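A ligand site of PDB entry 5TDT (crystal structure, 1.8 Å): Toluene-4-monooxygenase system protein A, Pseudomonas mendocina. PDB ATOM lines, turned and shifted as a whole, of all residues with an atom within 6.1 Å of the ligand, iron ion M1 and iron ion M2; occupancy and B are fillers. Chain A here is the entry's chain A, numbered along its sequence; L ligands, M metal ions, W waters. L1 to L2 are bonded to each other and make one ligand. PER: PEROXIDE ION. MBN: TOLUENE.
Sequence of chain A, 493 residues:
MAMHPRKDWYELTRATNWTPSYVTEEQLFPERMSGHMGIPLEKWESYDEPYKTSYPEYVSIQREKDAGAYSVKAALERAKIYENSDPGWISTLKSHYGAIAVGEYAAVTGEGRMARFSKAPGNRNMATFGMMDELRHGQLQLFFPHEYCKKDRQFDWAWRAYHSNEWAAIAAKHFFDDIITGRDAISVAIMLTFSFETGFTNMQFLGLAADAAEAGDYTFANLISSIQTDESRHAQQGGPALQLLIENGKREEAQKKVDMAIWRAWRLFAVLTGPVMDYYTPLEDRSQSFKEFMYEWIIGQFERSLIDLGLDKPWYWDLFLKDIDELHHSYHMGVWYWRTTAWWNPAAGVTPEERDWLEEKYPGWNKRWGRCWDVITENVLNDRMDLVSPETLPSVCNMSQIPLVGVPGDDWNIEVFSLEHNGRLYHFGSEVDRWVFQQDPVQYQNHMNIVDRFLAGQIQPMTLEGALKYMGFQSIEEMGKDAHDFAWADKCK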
ATOM      1  N   ALA A  99       6.120 -27.846 -19.768  1.00  0.00           N
ATOM      2  CA  ALA A  99       5.770 -26.687 -18.959  1.00  0.00           C
ATOM      3  C   ALA A  99       5.763 -26.971 -17.455  1.00  0.00           C
ATOM      4  O   ALA A  99       5.893 -26.025 -16.665  1.00  0.00           O
ATOM      5  CB  ALA A  99       4.402 -26.143 -19.396  1.00  0.00           C
ATOM      6  N   ILE A 100       5.648 -28.231 -17.034  1.00  0.00           N
ATOM      7  CA  ILE A 100       5.319 -28.571 -15.653  1.00  0.00           C
ATOM      8  C   ILE A 100       6.468 -29.271 -14.925  1.00  0.00           C
ATOM      9  O   ILE A 100       6.712 -28.967 -13.759  1.00  0.00           O
ATOM     10  CB  ILE A 100       4.023 -29.414 -15.609  1.00  0.00           C
ATOM     11  CG1 ILE A 100       2.806 -28.592 -16.062  1.00  0.00           C
ATOM     12  CG2 ILE A 100       3.790 -29.998 -14.203  1.00  0.00           C
ATOM     13  CD1 ILE A 100       2.576 -27.317 -15.274  1.00  0.00           C
ATOM     14  N   ALA A 101       7.146 -30.212 -15.574  1.00  0.00           N
ATOM     15  CA  ALA A 101       7.963 -31.185 -14.827  1.00  0.00           C
ATOM     16  C   ALA A 101       9.058 -30.512 -13.992  1.00  0.00           C
ATOM     17  O   ALA A 101       9.199 -30.780 -12.795  1.00  0.00           O
ATOM     18  CB  ALA A 101       8.568 -32.221 -15.770  1.00  0.00           C
ATOM     19  N   VAL A 102       9.859 -29.645 -14.611  1.00  0.00           N
ATOM     20  CA  VAL A 102      10.943 -29.041 -13.851  1.00  0.00           C
ATOM     21  C   VAL A 102      10.442 -27.883 -12.997  1.00  0.00           C
ATOM     22  O   VAL A 102      11.085 -27.527 -12.009  1.00  0.00           O
ATOM     23  CB  VAL A 102      12.077 -28.664 -14.839  1.00  0.00           C
ATOM     24  CG1 VAL A 102      13.247 -27.886 -14.141  1.00  0.00           C
ATOM     25  CG2 VAL A 102      12.605 -29.942 -15.494  1.00  0.00           C
ATOM     26  N   GLY A 103       9.266 -27.327 -13.306  1.00  0.00           N
ATOM     27  CA  GLY A 103       8.637 -26.364 -12.410  1.00  0.00           C
ATOM     28  C   GLY A 103       8.140 -27.003 -11.130  1.00  0.00           C
ATOM     29  O   GLY A 103       8.166 -26.387 -10.065  1.00  0.00           O
ATOM     30  N   GLU A 104       7.667 -28.251 -11.214  1.00  0.00           N
ATOM     31  CA  GLU A 104       7.369 -29.010 -10.000  1.00  0.00           C
ATOM     32  C   GLU A 104       8.608 -29.160  -9.134  1.00  0.00           C
ATOM     33  O   GLU A 104       8.555 -29.016  -7.910  1.00  0.00           O
ATOM     34  CB  GLU A 104       6.826 -30.392 -10.365  1.00  0.00           C
ATOM     35  CG  GLU A 104       5.534 -30.338 -11.124  1.00  0.00           C
ATOM     36  CD  GLU A 104       4.334 -30.629 -10.257  1.00  0.00           C
ATOM     37  OE1 GLU A 104       3.339 -31.150 -10.798  1.00  0.00           O
ATOM     38  OE2 GLU A 104       4.393 -30.359  -9.026  1.00  0.00           O
ATOM     39  N   ALA A 107       9.212 -26.183  -7.210  1.00  0.00           N
ATOM     40  CA  ALA A 107       8.322 -26.020  -6.065  1.00  0.00           C
ATOM     41  C   ALA A 107       8.902 -26.624  -4.791  1.00  0.00           C
ATOM     42  O   ALA A 107       8.514 -26.209  -3.690  1.00  0.00           O
ATOM     43  CB  ALA A 107       6.947 -26.632  -6.365  1.00  0.00           C
ATOM     44  N   GLU A 111       8.619 -24.847  -0.983  1.00  0.00           N
ATOM     45  CA  GLU A 111       8.320 -25.546   0.253  1.00  0.00           C
ATOM     46  C   GLU A 111       9.509 -25.501   1.220  1.00  0.00           C
ATOM     47  O   GLU A 111       9.339 -25.330   2.424  1.00  0.00           O
ATOM     48  CB  GLU A 111       7.936 -27.007  -0.053  1.00  0.00           C
ATOM     49  CG  GLU A 111       6.613 -27.182  -0.851  1.00  0.00           C
ATOM     50  CD  GLU A 111       5.344 -26.922  -0.031  1.00  0.00           C
ATOM     51  OE1 GLU A 111       5.430 -26.782   1.209  1.00  0.00           O
ATOM     52  OE2 GLU A 111       4.232 -26.883  -0.640  1.00  0.00           O
ATOM     53  N   ASP A 133       6.495 -34.029  -1.465  1.00  0.00           N
ATOM     54  CA  ASP A 133       5.471 -34.122  -2.514  1.00  0.00           C
ATOM     55  C   ASP A 133       6.000 -33.591  -3.838  1.00  0.00           C
ATOM     56  O   ASP A 133       5.786 -34.209  -4.898  1.00  0.00           O
ATOM     57  CB  ASP A 133       4.214 -33.346  -2.115  1.00  0.00           C
ATOM     58  CG  ASP A 133       3.469 -33.947  -0.941  1.00  0.00           C
ATOM     59  OD1 ASP A 133       3.681 -35.140  -0.575  1.00  0.00           O
ATOM     60  OD2 ASP A 133       2.635 -33.211  -0.382  1.00  0.00           O
ATOM     61  N   GLU A 134       6.649 -32.425  -3.826  1.00  0.00           N
ATOM     62  CA  GLU A 134       7.037 -31.853  -5.113  1.00  0.00           C
ATOM     63  C   GLU A 134       8.226 -32.608  -5.711  1.00  0.00           C
ATOM     64  O   GLU A 134       8.369 -32.657  -6.936  1.00  0.00           O
ATOM     65  CB  GLU A 134       7.344 -30.361  -4.979  1.00  0.00           C
ATOM     66  CG  GLU A 134       6.212 -29.537  -4.349  1.00  0.00           C
ATOM     67  CD  GLU A 134       4.943 -29.436  -5.210  1.00  0.00           C
ATOM     68  OE1 GLU A 134       4.750 -30.213  -6.186  1.00  0.00           O
ATOM     69  OE2 GLU A 134       4.116 -28.546  -4.904  1.00  0.00           O
ATOM     70  N   HIS A 137       6.478 -35.199  -7.602  1.00  0.00           N
ATOM     71  CA  HIS A 137       5.832 -34.716  -8.813  1.00  0.00           C
ATOM     72  C   HIS A 137       6.844 -34.428  -9.919  1.00  0.00           C
ATOM     73  O   HIS A 137       6.583 -34.726 -11.088  1.00  0.00           O
ATOM     74  CB  HIS A 137       4.992 -33.476  -8.504  1.00  0.00           C
ATOM     75  CG  HIS A 137       3.945 -33.720  -7.464  1.00  0.00           C
ATOM     76  ND1 HIS A 137       3.225 -32.711  -6.862  1.00  0.00           N
ATOM     77  CD2 HIS A 137       3.496 -34.881  -6.921  1.00  0.00           C
ATOM     78  CE1 HIS A 137       2.383 -33.232  -5.985  1.00  0.00           C
ATOM     79  NE2 HIS A 137       2.524 -34.556  -5.999  1.00  0.00           N
ATOM     80  N   GLN A 141       7.028 -36.742 -13.381  1.00  0.00           N
ATOM     81  CA  GLN A 141       6.766 -36.085 -14.653  1.00  0.00           C
ATOM     82  C   GLN A 141       8.012 -35.938 -15.512  1.00  0.00           C
ATOM     83  O   GLN A 141       7.910 -35.438 -16.640  1.00  0.00           O
ATOM     84  CB  GLN A 141       6.073 -34.753 -14.393  1.00  0.00           C
ATOM     85  CG  GLN A 141       4.633 -35.060 -14.010  1.00  0.00           C
ATOM     86  CD  GLN A 141       3.859 -33.878 -13.530  1.00  0.00           C
ATOM     87  OE1 GLN A 141       2.834 -33.518 -14.131  1.00  0.00           O
ATOM     88  NE2 GLN A 141       4.292 -33.287 -12.429  1.00  0.00           N
ATOM     89  N   TYR A 162      12.887 -25.815 -19.194  1.00  0.00           N
ATOM     90  CA  TYR A 162      13.245 -24.820 -18.185  1.00  0.00           C
ATOM     91  C   TYR A 162      14.714 -24.419 -18.264  1.00  0.00           C
ATOM     92  O   TYR A 162      15.117 -23.429 -17.653  1.00  0.00           O
ATOM     93  CB  TYR A 162      12.921 -25.342 -16.772  1.00  0.00           C
ATOM     94  CG  TYR A 162      11.462 -25.133 -16.343  1.00  0.00           C
ATOM     95  CD1 TYR A 162      10.436 -25.813 -16.987  1.00  0.00           C
ATOM     96  CD2 TYR A 162      11.139 -24.282 -15.291  1.00  0.00           C
ATOM     97  CE1 TYR A 162       9.095 -25.629 -16.604  1.00  0.00           C
ATOM     98  CE2 TYR A 162       9.810 -24.103 -14.881  1.00  0.00           C
ATOM     99  CZ  TYR A 162       8.800 -24.781 -15.543  1.00  0.00           C
ATOM    100  OH  TYR A 162       7.483 -24.598 -15.159  1.00  0.00           O
ATOM    101  N   PHE A 176       6.877 -18.684 -12.110  1.00  0.00           N
ATOM    102  CA  PHE A 176       7.237 -19.552 -10.996  1.00  0.00           C
ATOM    103  C   PHE A 176       8.380 -18.985 -10.158  1.00  0.00           C
ATOM    104  O   PHE A 176       8.390 -19.171  -8.932  1.00  0.00           O
ATOM    105  CB  PHE A 176       7.583 -20.958 -11.482  1.00  0.00           C
ATOM    106  CG  PHE A 176       6.400 -21.737 -11.976  1.00  0.00           C
ATOM    107  CD1 PHE A 176       5.220 -21.791 -11.230  1.00  0.00           C
ATOM    108  CD2 PHE A 176       6.423 -22.365 -13.198  1.00  0.00           C
ATOM    109  CE1 PHE A 176       4.114 -22.493 -11.688  1.00  0.00           C
ATOM    110  CE2 PHE A 176       5.326 -23.062 -13.659  1.00  0.00           C
ATOM    111  CZ  PHE A 176       4.170 -23.118 -12.912  1.00  0.00           C
ATOM    112  N   ILE A 180       7.105 -18.745  -6.501  1.00  0.00           N
ATOM    113  CA  ILE A 180       7.606 -19.936  -5.808  1.00  0.00           C
ATOM    114  C   ILE A 180       8.985 -19.687  -5.176  1.00  0.00           C
ATOM    115  O   ILE A 180       9.163 -19.863  -3.968  1.00  0.00           O
ATOM    116  CB  ILE A 180       7.646 -21.170  -6.737  1.00  0.00           C
ATOM    117  CG1 ILE A 180       6.242 -21.519  -7.220  1.00  0.00           C
ATOM    118  CG2 ILE A 180       8.307 -22.344  -6.001  1.00  0.00           C
ATOM    119  CD1 ILE A 180       6.183 -22.774  -8.054  1.00  0.00           C
ATOM    120  N   LEU A 192       1.721 -19.304  -3.629  1.00  0.00           N
ATOM    121  CA  LEU A 192       1.833 -20.664  -4.169  1.00  0.00           C
ATOM    122  C   LEU A 192       0.729 -21.551  -3.597  1.00  0.00           C
ATOM    123  O   LEU A 192      -0.171 -21.973  -4.328  1.00  0.00           O
ATOM    124  CB  LEU A 192       3.212 -21.246  -3.866  1.00  0.00           C
ATOM    125  CG  LEU A 192       3.382 -22.753  -4.159  1.00  0.00           C
ATOM    126  CD1 LEU A 192       3.137 -23.078  -5.640  1.00  0.00           C
ATOM    127  CD2 LEU A 192       4.761 -23.240  -3.739  1.00  0.00           C
ATOM    128  N   PHE A 196      -2.255 -20.412  -6.226  1.00  0.00           N
ATOM    129  CA  PHE A 196      -1.989 -21.278  -7.365  1.00  0.00           C
ATOM    130  C   PHE A 196      -2.467 -22.713  -7.104  1.00  0.00           C
ATOM    131  O   PHE A 196      -3.114 -23.326  -7.960  1.00  0.00           O
ATOM    132  CB  PHE A 196      -0.500 -21.253  -7.677  1.00  0.00           C
ATOM    133  CG  PHE A 196      -0.101 -22.052  -8.875  1.00  0.00           C
ATOM    134  CD1 PHE A 196      -0.607 -21.722 -10.132  1.00  0.00           C
ATOM    135  CD2 PHE A 196       0.792 -23.103  -8.763  1.00  0.00           C
ATOM    136  CE1 PHE A 196      -0.234 -22.469 -11.253  1.00  0.00           C
ATOM    137  CE2 PHE A 196       1.161 -23.834  -9.869  1.00  0.00           C
ATOM    138  CZ  PHE A 196       0.655 -23.519 -11.117  1.00  0.00           C
ATOM    139  N   GLU A 197      -2.187 -23.255  -5.907  1.00  0.00           N
ATOM    140  CA  GLU A 197      -2.354 -24.687  -5.672  1.00  0.00           C
ATOM    141  C   GLU A 197      -3.771 -25.093  -5.240  1.00  0.00           C
ATOM    142  O   GLU A 197      -4.130 -26.266  -5.427  1.00  0.00           O
ATOM    143  CB  GLU A 197      -1.345 -25.188  -4.647  1.00  0.00           C
ATOM    144  CG  GLU A 197       0.096 -25.155  -5.191  1.00  0.00           C
ATOM    145  CD  GLU A 197       1.128 -25.811  -4.281  1.00  0.00           C
ATOM    146  OE1 GLU A 197       1.085 -25.618  -3.052  1.00  0.00           O
ATOM    147  OE2 GLU A 197       1.995 -26.537  -4.797  1.00  0.00           O
ATOM    148  N   THR A 201      -4.218 -25.058 -10.346  1.00  0.00           N
ATOM    149  CA  THR A 201      -3.694 -26.348 -10.790  1.00  0.00           C
ATOM    150  C   THR A 201      -4.798 -27.371 -11.030  1.00  0.00           C
ATOM    151  O   THR A 201      -4.615 -28.315 -11.804  1.00  0.00           O
ATOM    152  CB  THR A 201      -2.672 -26.920  -9.806  1.00  0.00           C
ATOM    153  OG1 THR A 201      -3.267 -27.022  -8.507  1.00  0.00           O
ATOM    154  CG2 THR A 201      -1.426 -26.025  -9.741  1.00  0.00           C
ATOM    155  N   PHE A 205      -4.589 -30.363 -13.839  1.00  0.00           N
ATOM    156  CA  PHE A 205      -4.397 -31.711 -13.326  1.00  0.00           C
ATOM    157  C   PHE A 205      -5.687 -32.499 -13.141  1.00  0.00           C
ATOM    158  O   PHE A 205      -5.620 -33.720 -12.927  1.00  0.00           O
ATOM    159  CB  PHE A 205      -3.637 -31.674 -11.993  1.00  0.00           C
ATOM    160  CG  PHE A 205      -2.181 -31.365 -12.150  1.00  0.00           C
ATOM    161  CD1 PHE A 205      -1.762 -30.052 -12.363  1.00  0.00           C
ATOM    162  CD2 PHE A 205      -1.237 -32.372 -12.096  1.00  0.00           C
ATOM    163  CE1 PHE A 205      -0.399 -29.755 -12.503  1.00  0.00           C
ATOM    164  CE2 PHE A 205       0.116 -32.087 -12.245  1.00  0.00           C
ATOM    165  CZ  PHE A 205       0.532 -30.765 -12.456  1.00  0.00           C
ATOM    166  N   ILE A 227      -1.254 -37.150  -8.599  1.00  0.00           N
ATOM    167  CA  ILE A 227      -0.456 -36.009  -8.191  1.00  0.00           C
ATOM    168  C   ILE A 227      -1.331 -35.001  -7.454  1.00  0.00           C
ATOM    169  O   ILE A 227      -0.957 -34.462  -6.402  1.00  0.00           O
ATOM    170  CB  ILE A 227       0.224 -35.399  -9.435  1.00  0.00           C
ATOM    171  CG1 ILE A 227       1.394 -36.293  -9.861  1.00  0.00           C
ATOM    172  CG2 ILE A 227       0.644 -33.948  -9.180  1.00  0.00           C
ATOM    173  CD1 ILE A 227       2.011 -35.891 -11.203  1.00  0.00           C
ATOM    174  N   ASP A 230      -1.861 -35.183  -3.660  1.00  0.00           N
ATOM    175  CA  ASP A 230      -0.853 -34.539  -2.814  1.00  0.00           C
ATOM    176  C   ASP A 230      -1.100 -33.038  -2.721  1.00  0.00           C
ATOM    177  O   ASP A 230      -1.006 -32.447  -1.635  1.00  0.00           O
ATOM    178  CB  ASP A 230       0.575 -34.787  -3.359  1.00  0.00           C
ATOM    179  CG  ASP A 230       0.938 -36.269  -3.467  1.00  0.00           C
ATOM    180  OD1 ASP A 230       1.619 -36.617  -4.442  1.00  0.00           O
ATOM    181  OD2 ASP A 230       0.553 -37.071  -2.578  1.00  0.00           O
ATOM    182  N   GLU A 231      -1.319 -32.407  -3.873  1.00  0.00           N
ATOM    183  CA  GLU A 231      -1.602 -30.972  -3.919  1.00  0.00           C
ATOM    184  C   GLU A 231      -2.703 -30.610  -2.933  1.00  0.00           C
ATOM    185  O   GLU A 231      -2.579 -29.631  -2.179  1.00  0.00           O
ATOM    186  CB  GLU A 231      -1.998 -30.578  -5.346  1.00  0.00           C
ATOM    187  CG  GLU A 231      -2.287 -29.100  -5.516  1.00  0.00           C
ATOM    188  CD  GLU A 231      -1.058 -28.315  -5.918  1.00  0.00           C
ATOM    189  OE1 GLU A 231      -1.080 -27.664  -6.988  1.00  0.00           O
ATOM    190  OE2 GLU A 231      -0.069 -28.367  -5.168  1.00  0.00           O
ATOM    191  N   HIS A 234      -1.039 -30.442   0.695  1.00  0.00           N
ATOM    192  CA  HIS A 234      -0.082 -29.401   1.092  1.00  0.00           C
ATOM    193  C   HIS A 234      -0.524 -27.998   0.667  1.00  0.00           C
ATOM    194  O   HIS A 234      -0.012 -27.023   1.226  1.00  0.00           O
ATOM    195  CB  HIS A 234       1.348 -29.710   0.590  1.00  0.00           C
ATOM    196  CG  HIS A 234       1.532 -29.669  -0.892  1.00  0.00           C
ATOM    197  ND1 HIS A 234       2.004 -30.754  -1.608  1.00  0.00           N
ATOM    198  CD2 HIS A 234       1.395 -28.661  -1.790  1.00  0.00           C
ATOM    199  CE1 HIS A 234       2.102 -30.433  -2.891  1.00  0.00           C
ATOM    200  NE2 HIS A 234       1.739 -29.162  -3.020  1.00  0.00           N
ATOM    201  N   ALA A 235      -1.490 -27.875  -0.247  1.00  0.00           N
ATOM    202  CA  ALA A 235      -2.068 -26.563  -0.518  1.00  0.00           C
ATOM    203  C   ALA A 235      -2.821 -26.000   0.694  1.00  0.00           C
ATOM    204  O   ALA A 235      -3.004 -24.791   0.784  1.00  0.00           O
ATOM    205  CB  ALA A 235      -3.016 -26.611  -1.725  1.00  0.00           C
HETATM  206  O1  PER L   1       2.381 -28.166  -7.925  1.00  0.00           O
HETATM  207  O2  PER L   1       3.582 -27.886  -7.242  1.00  0.00           O
HETATM  208  C   MBN L   2       4.655 -26.391 -12.380  1.00  0.00           C
HETATM  209  C1  MBN L   2       3.928 -26.612 -11.067  1.00  0.00           C
HETATM  210  C2  MBN L   2       4.492 -26.113  -9.906  1.00  0.00           C
HETATM  211  C3  MBN L   2       3.836 -26.295  -8.706  1.00  0.00           C
HETATM  212  C4  MBN L   2       2.647 -27.019  -8.643  1.00  0.00           C
HETATM  213  C5  MBN L   2       2.091 -27.520  -9.819  1.00  0.00           C
HETATM  214  C6  MBN L   2       2.731 -27.317 -11.030  1.00  0.00           C
HETATM  215 FE    FE M   1       3.124 -30.532  -7.408  1.00  0.00          FE
HETATM  216 FE    FE M   2       2.008 -28.451  -5.161  1.00  0.00          FE
HETATM  217  O   HOH W   1       1.595 -30.130  -5.970  1.00  0.00           O
HETATM  218  O   HOH W   2       1.662 -30.928  -8.762  1.00  0.00           O
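The side-chain hydroxyl (OG1) of Thr 201 sits at hydrogen-bond distance from the backbone carbonyl oxygen (O) of Glu 197.
The backbone carbonyl oxygen (O) of Leu 192 is in hydrogen-bond range of the backbone NH (N) of Glu 197 (2.9 Å).
OE1 of Glu 231 lies within hydrogen-bond range of OG1 of Thr 201 (2.7 Å).
NE2 of His 137 lies close to O of Asp 133 (3.5 Å).
OD1 of Asp 230 sits at hydrogen-bond distance from NE2 of His 137 (2.7 Å).
A ring nitrogen (ND1) of His 234 lies within hydrogen-bond range of the side-chain carboxylate (OD2) of Asp 133.
The backbone carbonyl oxygen (O) of Asp 230 lies within hydrogen-bond range of a ring nitrogen (ND1) of His 234, at 3.5 Å.
The backbone carbonyl oxygen (O) of Phe 196 sits at hydrogen-bond distance from the backbone NH (N) of Thr 201 (3.1 Å).
O of Ile 100 touches C of MBN L2, at 3.6 Å.
O of Gly 103 touches C2 of MBN L2, 3.7 Å away.
Ala 107 touches the ligand.
Phe 176 touches the ligand.
CE2 of Phe 196 touches C4 of MBN L2, 3.7 Å away.
Thr 201 touches the ligand.
Hydrophobic or aromatic side chains that line the ligand: Ile 100, Ala 107, Phe 176 and Phe 196.
Of the 25 residues printed, 10 come within 4 Å of the ligand.
The nearest printed residue that does not touch the ligand is Ile 180 (4.2 Å).
The nearest printed residue that does not touch iron ion M1 is Glu 231 (4.5 Å).
Within 4 Å of iron ion M2: Glu 134, Glu 197, Glu 231 and His 234.
The nearest printed residue that does not touch iron ion M2 is His 137 (4.7 Å).
Iron ion M1 is bound by water W2 (2.0 Å), OE1 of Glu 134 (2.1 Å), OE2 of Glu 104 (2.1 Å), water W1 (2.1 Å), ND1 of His 137 (2.2 Å) and O1 of PER L1 (2.5 Å).
Iron ion M1 has six donor atoms within binding distance.
Iron ion M2 is bound by water W1 (1.9 Å), OE2 of Glu 197 (1.9 Å), OE2 of Glu 231 (2.1 Å), OE2 of Glu 134 (2.1 Å) and NE2 of His 234 (2.3 Å).
Iron ion M2 has five donor atoms within binding distance.
Slightly farther from iron ion M2 lies an oxygen (O2) of PER L1 (2.7 Å).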
